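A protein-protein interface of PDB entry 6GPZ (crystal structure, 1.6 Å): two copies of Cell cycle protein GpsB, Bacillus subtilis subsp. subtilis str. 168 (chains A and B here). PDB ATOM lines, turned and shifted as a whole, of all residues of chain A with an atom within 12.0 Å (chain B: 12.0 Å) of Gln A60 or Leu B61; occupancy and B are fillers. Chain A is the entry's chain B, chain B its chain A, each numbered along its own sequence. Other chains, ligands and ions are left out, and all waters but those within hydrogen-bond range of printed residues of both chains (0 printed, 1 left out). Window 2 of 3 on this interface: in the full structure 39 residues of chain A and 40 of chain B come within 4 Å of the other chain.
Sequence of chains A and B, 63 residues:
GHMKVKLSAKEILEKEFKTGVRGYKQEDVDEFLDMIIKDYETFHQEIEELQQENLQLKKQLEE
OD1 of Asn B54 sits at hydrogen-bond distance from ND2 of Asn A54 (2.9 Å).
Glu A53 touches Asn B54, and with the chains exchanged Asn A54 touches Glu B53.
Asn A54 touches Leu B57, and with the chains exchanged Leu A57 touches Asn B54.
Leu A57 touches Leu B61, and with the chains exchanged Leu A61 touches Leu B57.
Gln A60 touches Leu B61, and with the chains exchanged Leu A61 touches Gln B60.
Positions printed for both chains: 52, 53, 54, 55, 56, 57, 58, 59, 60, 61 and 62.
Of the 11 pairs that touch across the chains among the printed residues, 10 have their exchanged pair printed and touching as well.
Gln A60 touches just one residue of chain B: Leu B61.
Leu B61 touches just these residues of chain A: Leu A57 and Gln A60.
Gln A56 touches none of the printed residues of chain B.
Of chain B, only Asn B54 (3.6 Å), Leu B57 (3.9 Å), Lys B58 (3.8 Å) and Leu B61 (3.6 Å) come within 4 Å of Leu A57.
No residue of chain B comes within 4 Å of Lys A59.
Leu A61 touches just these residues of chain B: Leu B57 (3.6 Å) and Gln B60 (3.9 Å).
Leu B57 touches just these residues of chain A: Asn A54 (3.7 Å), Leu A57 (3.9 Å) and Leu A61 (3.6 Å).
Lys B58 touches just one residue of chain A: Leu A57.
Gln B60 touches just one residue of chain A: Leu A61.
No residue of chain A comes within 4 Å of Glu B62.
Of the printed residues of chain B, Asn A54 touches Glu B53 (3.996 Å), Asn B54 (2.9 Å) and Leu B57 (3.7 Å).
Of the printed residues of chain A, Asn B54 touches Glu A53 (3.8 Å), Asn A54 (2.9 Å) and Leu A57 (3.6 Å).
Printed residues of chain A within 4 Å of Glu B53: Asn A54.
Leu A55 touches none of the printed residues of chain B.
The nearest residue of chain B that does not touch Gln A60 is Leu B57 (7.3 Å).
Of the 12 printed residues of chain B, 6 touch a printed residue of chain A.
Hydrophobic or aromatic side chains of chain B within 4 Å of the printed part of chain A: Leu B57 and Leu B61.
Hydrophobic or aromatic side chains of chain A that line the printed part of chain B: Leu A57 and Leu A61.
Among the printed residues, 11 pairs touch across the chains.
Among the printed residues, no Asp or Glu carboxylate lies within 4 Å of a Lys or Arg side-chain nitrogen of the other chain.
Among the printed residues, pairs that only touch across the chains: Glu A53 with Asn B54 (3.8 Å), Asn A54 with Glu B53 (3.996 Å), Asn A54 with Leu B57 (3.7 Å), Leu A57 with Asn B54 (3.6 Å), Leu A57 with Leu B57 (3.9 Å), Leu A57 with Lys B58 (3.8 Å), Leu A57 with Leu B61 (3.6 Å), Gln A60 with Leu B61 (3.7 Å), Leu A61 with Leu B57 (3.6 Å) and Leu A61 with Gln B60 (3.9 Å).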
ATOM      1  N   GLN A  51      12.099 -17.366 -19.993  1.00  0.00           N
ATOM      2  CA  GLN A  51      13.266 -17.556 -20.881  1.00  0.00           C
ATOM      3  C   GLN A  51      12.895 -17.431 -22.366  1.00  0.00           C
ATOM      4  O   GLN A  51      13.687 -16.912 -23.158  1.00  0.00           O
ATOM      5  CB  GLN A  51      13.942 -18.913 -20.623  1.00  0.00           C
ATOM      6  CG  GLN A  51      14.730 -18.942 -19.310  1.00  0.00           C
ATOM      7  CD  GLN A  51      15.367 -20.300 -18.904  1.00  0.00           C
ATOM      8  OE1 GLN A  51      16.229 -20.340 -18.005  1.00  0.00           O
ATOM      9  NE2 GLN A  51      14.956 -21.391 -19.546  1.00  0.00           N
ATOM     10  N   GLN A  52      11.717 -17.903 -22.772  1.00  0.00           N
ATOM     11  CA  GLN A  52      11.292 -17.701 -24.155  1.00  0.00           C
ATOM     12  C   GLN A  52      11.110 -16.218 -24.456  1.00  0.00           C
ATOM     13  O   GLN A  52      11.434 -15.763 -25.553  1.00  0.00           O
ATOM     14  CB  GLN A  52      10.002 -18.475 -24.423  1.00  0.00           C
ATOM     15  CG  GLN A  52       9.562 -18.441 -25.861  1.00  0.00           C
ATOM     16  N   GLU A  53      10.612 -15.449 -23.478  1.00  0.00           N
ATOM     17  CA  GLU A  53      10.463 -14.011 -23.666  1.00  0.00           C
ATOM     18  C   GLU A  53      11.824 -13.342 -23.762  1.00  0.00           C
ATOM     19  O   GLU A  53      12.029 -12.481 -24.623  1.00  0.00           O
ATOM     20  CB  GLU A  53       9.630 -13.402 -22.528  1.00  0.00           C
ATOM     21  CG  GLU A  53       8.113 -13.577 -22.729  1.00  0.00           C
ATOM     22  CD  GLU A  53       7.246 -13.284 -21.493  1.00  0.00           C
ATOM     23  OE1 GLU A  53       6.043 -13.654 -21.493  1.00  0.00           O
ATOM     24  OE2 GLU A  53       7.759 -12.679 -20.527  1.00  0.00           O
ATOM     25  N   ASN A  54      12.759 -13.743 -22.899  1.00  0.00           N
ATOM     26  CA  ASN A  54      14.131 -13.236 -22.915  1.00  0.00           C
ATOM     27  C   ASN A  54      14.785 -13.469 -24.270  1.00  0.00           C
ATOM     28  O   ASN A  54      15.452 -12.574 -24.813  1.00  0.00           O
ATOM     29  CB  ASN A  54      14.911 -13.931 -21.796  1.00  0.00           C
ATOM     30  CG  ASN A  54      16.316 -13.414 -21.622  1.00  0.00           C
ATOM     31  OD1 ASN A  54      17.266 -14.099 -21.989  1.00  0.00           O
ATOM     32  ND2 ASN A  54      16.459 -12.218 -21.067  1.00  0.00           N
ATOM     33  N   LEU A  55      14.624 -14.676 -24.824  1.00  0.00           N
ATOM     34  CA  LEU A  55      15.158 -14.954 -26.159  1.00  0.00           C
ATOM     35  C   LEU A  55      14.554 -14.033 -27.210  1.00  0.00           C
ATOM     36  O   LEU A  55      15.276 -13.512 -28.079  1.00  0.00           O
ATOM     37  CB  LEU A  55      14.914 -16.408 -26.561  1.00  0.00           C
ATOM     38  CG  LEU A  55      15.870 -17.446 -25.987  1.00  0.00           C
ATOM     39  CD1 LEU A  55      15.540 -18.820 -26.532  1.00  0.00           C
ATOM     40  CD2 LEU A  55      17.298 -17.105 -26.342  1.00  0.00           C
ATOM     41  N   GLN A  56      13.240 -13.805 -27.156  1.00  0.00           N
ATOM     42  CA  GLN A  56      12.606 -12.928 -28.147  1.00  0.00           C
ATOM     43  C   GLN A  56      13.131 -11.490 -28.040  1.00  0.00           C
ATOM     44  O   GLN A  56      13.419 -10.842 -29.061  1.00  0.00           O
ATOM     45  CB  GLN A  56      11.082 -12.977 -27.977  1.00  0.00           C
ATOM     46  N   LEU A  57      13.268 -10.973 -26.810  1.00  0.00           N
ATOM     47  CA  LEU A  57      13.739  -9.599 -26.610  1.00  0.00           C
ATOM     48  C   LEU A  57      15.175  -9.418 -27.099  1.00  0.00           C
ATOM     49  O   LEU A  57      15.511  -8.418 -27.767  1.00  0.00           O
ATOM     50  CB  LEU A  57      13.611  -9.259 -25.128  1.00  0.00           C
ATOM     51  CG  LEU A  57      12.183  -9.047 -24.698  1.00  0.00           C
ATOM     52  CD1 LEU A  57      12.135  -9.054 -23.149  1.00  0.00           C
ATOM     53  CD2 LEU A  57      11.660  -7.773 -25.294  1.00  0.00           C
ATOM     54  N   LYS A  58      16.043 -10.378 -26.765  1.00  0.00           N
ATOM     55  CA  LYS A  58      17.426 -10.336 -27.228  1.00  0.00           C
ATOM     56  C   LYS A  58      17.505 -10.418 -28.733  1.00  0.00           C
ATOM     57  O   LYS A  58      18.412  -9.819 -29.345  1.00  0.00           O
ATOM     58  CB  LYS A  58      18.211 -11.492 -26.600  1.00  0.00           C
ATOM     59  CG  LYS A  58      18.559 -11.303 -25.125  1.00  0.00           C
ATOM     60  CD  LYS A  58      19.079 -12.569 -24.516  1.00  0.00           C
ATOM     61  N   LYS A  59      16.557 -11.123 -29.358  1.00  0.00           N
ATOM     62  CA  LYS A  59      16.575 -11.179 -30.824  1.00  0.00           C
ATOM     63  C   LYS A  59      16.187  -9.845 -31.446  1.00  0.00           C
ATOM     64  O   LYS A  59      16.801  -9.422 -32.436  1.00  0.00           O
ATOM     65  CB  LYS A  59      15.669 -12.295 -31.332  1.00  0.00           C
ATOM     66  N   GLN A  60      15.167  -9.163 -30.908  1.00  0.00           N
ATOM     67  CA  GLN A  60      14.823  -7.850 -31.456  1.00  0.00           C
ATOM     68  C   GLN A  60      15.997  -6.875 -31.341  1.00  0.00           C
ATOM     69  O   GLN A  60      16.221  -6.036 -32.226  1.00  0.00           O
ATOM     70  CB  GLN A  60      13.588  -7.281 -30.753  1.00  0.00           C
ATOM     71  CG  GLN A  60      12.303  -8.143 -30.855  1.00  0.00           C
ATOM     72  N   LEU A  61      16.760  -6.974 -30.255  1.00  0.00           N
ATOM     73  CA  LEU A  61      17.871  -6.069 -29.992  1.00  0.00           C
ATOM     74  C   LEU A  61      19.093  -6.417 -30.831  1.00  0.00           C
ATOM     75  O   LEU A  61      19.955  -5.554 -31.034  1.00  0.00           O
ATOM     76  CB  LEU A  61      18.197  -6.076 -28.481  1.00  0.00           C
ATOM     77  CG  LEU A  61      17.289  -5.095 -27.735  1.00  0.00           C
ATOM     78  CD1 LEU A  61      17.251  -5.441 -26.261  1.00  0.00           C
ATOM     79  CD2 LEU A  61      17.748  -3.648 -27.893  1.00  0.00           C
ATOM     80  N   GLU A  62      19.164  -7.639 -31.349  1.00  0.00           N
ATOM     81  CA  GLU A  62      20.150  -8.013 -32.341  1.00  0.00           C
ATOM     82  C   GLU A  62      19.624  -7.674 -33.728  1.00  0.00           C
ATOM     83  O   GLU A  62      20.428  -7.380 -34.611  1.00  0.00           O
ATOM     84  CB  GLU A  62      20.474  -9.496 -32.256  1.00  0.00           C
ATOM     85  CG  GLU A  62      21.408  -9.855 -31.090  1.00  0.00           C
ATOM     86  CD  GLU A  62      22.870  -9.656 -31.477  1.00  0.00           C
ATOM     87  OE1 GLU A  62      23.411  -8.539 -31.290  1.00  0.00           O
ATOM     88  OE2 GLU A  62      23.472 -10.614 -32.002  1.00  0.00           O
ATOM     89  N   GLN B  52      13.995  -9.008 -14.200  1.00  0.00           N
ATOM     90  CA  GLN B  52      14.647  -7.707 -14.294  1.00  0.00           C
ATOM     91  C   GLN B  52      15.368  -7.563 -15.623  1.00  0.00           C
ATOM     92  O   GLN B  52      15.363  -6.480 -16.226  1.00  0.00           O
ATOM     93  CB  GLN B  52      15.614  -7.520 -13.130  1.00  0.00           C
ATOM     94  CG  GLN B  52      14.906  -7.283 -11.788  1.00  0.00           C
ATOM     95  N   GLU B  53      15.987  -8.645 -16.098  1.00  0.00           N
ATOM     96  CA  GLU B  53      16.621  -8.632 -17.414  1.00  0.00           C
ATOM     97  C   GLU B  53      15.602  -8.316 -18.499  1.00  0.00           C
ATOM     98  O   GLU B  53      15.871  -7.510 -19.382  1.00  0.00           O
ATOM     99  CB  GLU B  53      17.289  -9.993 -17.667  1.00  0.00           C
ATOM    100  CG  GLU B  53      18.722 -10.077 -17.108  1.00  0.00           C
ATOM    101  CD  GLU B  53      19.362 -11.466 -17.184  1.00  0.00           C
ATOM    102  OE1 GLU B  53      20.437 -11.659 -16.572  1.00  0.00           O
ATOM    103  OE2 GLU B  53      18.780 -12.366 -17.817  1.00  0.00           O
ATOM    104  N   ASN B  54      14.421  -8.959 -18.446  1.00  0.00           N
ATOM    105  CA  ASN B  54      13.425  -8.719 -19.492  1.00  0.00           C
ATOM    106  C   ASN B  54      12.885  -7.297 -19.421  1.00  0.00           C
ATOM    107  O   ASN B  54      12.588  -6.683 -20.454  1.00  0.00           O
ATOM    108  CB  ASN B  54      12.286  -9.735 -19.356  1.00  0.00           C
ATOM    109  CG  ASN B  54      12.667 -11.117 -19.844  1.00  0.00           C
ATOM    110  OD1 ASN B  54      13.756 -11.331 -20.334  1.00  0.00           O
ATOM    111  ND2 ASN B  54      11.755 -12.077 -19.674  1.00  0.00           N
ATOM    112  N   LEU B  55      12.711  -6.771 -18.208  1.00  0.00           N
ATOM    113  CA  LEU B  55      12.297  -5.376 -18.063  1.00  0.00           C
ATOM    114  C   LEU B  55      13.303  -4.455 -18.720  1.00  0.00           C
ATOM    115  O   LEU B  55      12.938  -3.513 -19.431  1.00  0.00           O
ATOM    116  CB  LEU B  55      12.148  -5.020 -16.577  1.00  0.00           C
ATOM    117  CG  LEU B  55      11.723  -3.562 -16.385  1.00  0.00           C
ATOM    118  CD1 LEU B  55      10.367  -3.398 -17.000  1.00  0.00           C
ATOM    119  CD2 LEU B  55      11.668  -3.208 -14.908  1.00  0.00           C
ATOM    120  N   GLN B  56      14.585  -4.704 -18.462  1.00  0.00           N
ATOM    121  CA  GLN B  56      15.626  -3.831 -18.979  1.00  0.00           C
ATOM    122  C   GLN B  56      15.662  -3.880 -20.502  1.00  0.00           C
ATOM    123  O   GLN B  56      15.902  -2.856 -21.155  1.00  0.00           O
ATOM    124  CB  GLN B  56      16.983  -4.225 -18.380  1.00  0.00           C
ATOM    125  N   LEU B  57      15.412  -5.065 -21.087  1.00  0.00           N
ATOM    126  CA  LEU B  57      15.488  -5.169 -22.548  1.00  0.00           C
ATOM    127  C   LEU B  57      14.266  -4.544 -23.203  1.00  0.00           C
ATOM    128  O   LEU B  57      14.364  -3.951 -24.286  1.00  0.00           O
ATOM    129  CB  LEU B  57      15.629  -6.627 -22.978  1.00  0.00           C
ATOM    130  CG  LEU B  57      16.841  -7.365 -22.448  1.00  0.00           C
ATOM    131  CD1 LEU B  57      16.586  -8.867 -22.592  1.00  0.00           C
ATOM    132  CD2 LEU B  57      18.157  -6.941 -23.155  1.00  0.00           C
ATOM    133  N   LYS B  58      13.118  -4.650 -22.558  1.00  0.00           N
ATOM    134  CA  LYS B  58      11.921  -4.008 -23.052  1.00  0.00           C
ATOM    135  C   LYS B  58      12.097  -2.502 -23.061  1.00  0.00           C
ATOM    136  O   LYS B  58      11.818  -1.850 -24.065  1.00  0.00           O
ATOM    137  CB  LYS B  58      10.738  -4.416 -22.166  1.00  0.00           C
ATOM    138  CG  LYS B  58       9.872  -5.499 -22.772  1.00  0.00           C
ATOM    139  N   LYS B  59      12.614  -1.938 -21.962  1.00  0.00           N
ATOM    140  CA  LYS B  59      12.839  -0.489 -21.898  1.00  0.00           C
ATOM    141  C   LYS B  59      13.822  -0.013 -22.958  1.00  0.00           C
ATOM    142  O   LYS B  59      13.647   1.055 -23.543  1.00  0.00           O
ATOM    143  CB  LYS B  59      13.345  -0.109 -20.509  1.00  0.00           C
ATOM    144  N   GLN B  60      14.879  -0.770 -23.192  1.00  0.00           N
ATOM    145  CA  GLN B  60      15.853  -0.344 -24.177  1.00  0.00           C
ATOM    146  C   GLN B  60      15.249  -0.353 -25.581  1.00  0.00           C
ATOM    147  O   GLN B  60      15.478   0.571 -26.371  1.00  0.00           O
ATOM    148  CB  GLN B  60      17.077  -1.239 -24.046  1.00  0.00           C
ATOM    149  CG  GLN B  60      18.203  -0.862 -24.959  1.00  0.00           C
ATOM    150  CD  GLN B  60      19.513  -1.486 -24.553  1.00  0.00           C
ATOM    151  OE1 GLN B  60      20.511  -0.791 -24.314  1.00  0.00           O
ATOM    152  NE2 GLN B  60      19.520  -2.808 -24.469  1.00  0.00           N
ATOM    153  N   LEU B  61      14.407  -1.352 -25.891  1.00  0.00           N
ATOM    154  CA  LEU B  61      13.788  -1.425 -27.216  1.00  0.00           C
ATOM    155  C   LEU B  61      13.013  -0.160 -27.529  1.00  0.00           C
ATOM    156  O   LEU B  61      12.941   0.263 -28.693  1.00  0.00           O
ATOM    157  CB  LEU B  61      12.847  -2.638 -27.307  1.00  0.00           C
ATOM    158  CG  LEU B  61      13.403  -3.932 -27.902  1.00  0.00           C
ATOM    159  CD1 LEU B  61      12.506  -5.137 -27.638  1.00  0.00           C
ATOM    160  CD2 LEU B  61      13.685  -3.826 -29.404  1.00  0.00           C
ATOM    161  N   GLU B  62      12.469   0.492 -26.512  1.00  0.00           N
ATOM    162  CA  GLU B  62      11.648   1.659 -26.758  1.00  0.00           C
ATOM    163  C   GLU B  62      12.326   2.969 -26.374  1.00  0.00           C
ATOM    164  O   GLU B  62      11.823   4.030 -26.747  1.00  0.00           O
ATOM    165  CB  GLU B  62      10.302   1.512 -26.028  1.00  0.00           C
ATOM    166  CG  GLU B  62       9.534   0.155 -26.295  1.00  0.00           C
ATOM    167  CD  GLU B  62       9.247  -0.223 -27.795  1.00  0.00           C
ATOM    168  OE1 GLU B  62       9.033   0.659 -28.673  1.00  0.00           O
ATOM    169  OE2 GLU B  62       9.177  -1.440 -28.088  1.00  0.00           O
ATOM    170  N   GLU B  63      13.492   2.932 -25.724  1.00  0.00           N
ATOM    171  CA  GLU B  63      14.226   4.161 -25.364  1.00  0.00           C
ATOM    172  C   GLU B  63      15.606   4.261 -26.058  1.00  0.00           C
ATOM    173  O   GLU B  63      15.681   4.509 -27.253  1.00  0.00           O
ATOM    174  CB  GLU B  63      14.377   4.241 -23.828  1.00  0.00           C
ATOM    175  OXT GLU B  63      16.695   4.129 -25.499  1.00  0.00           O
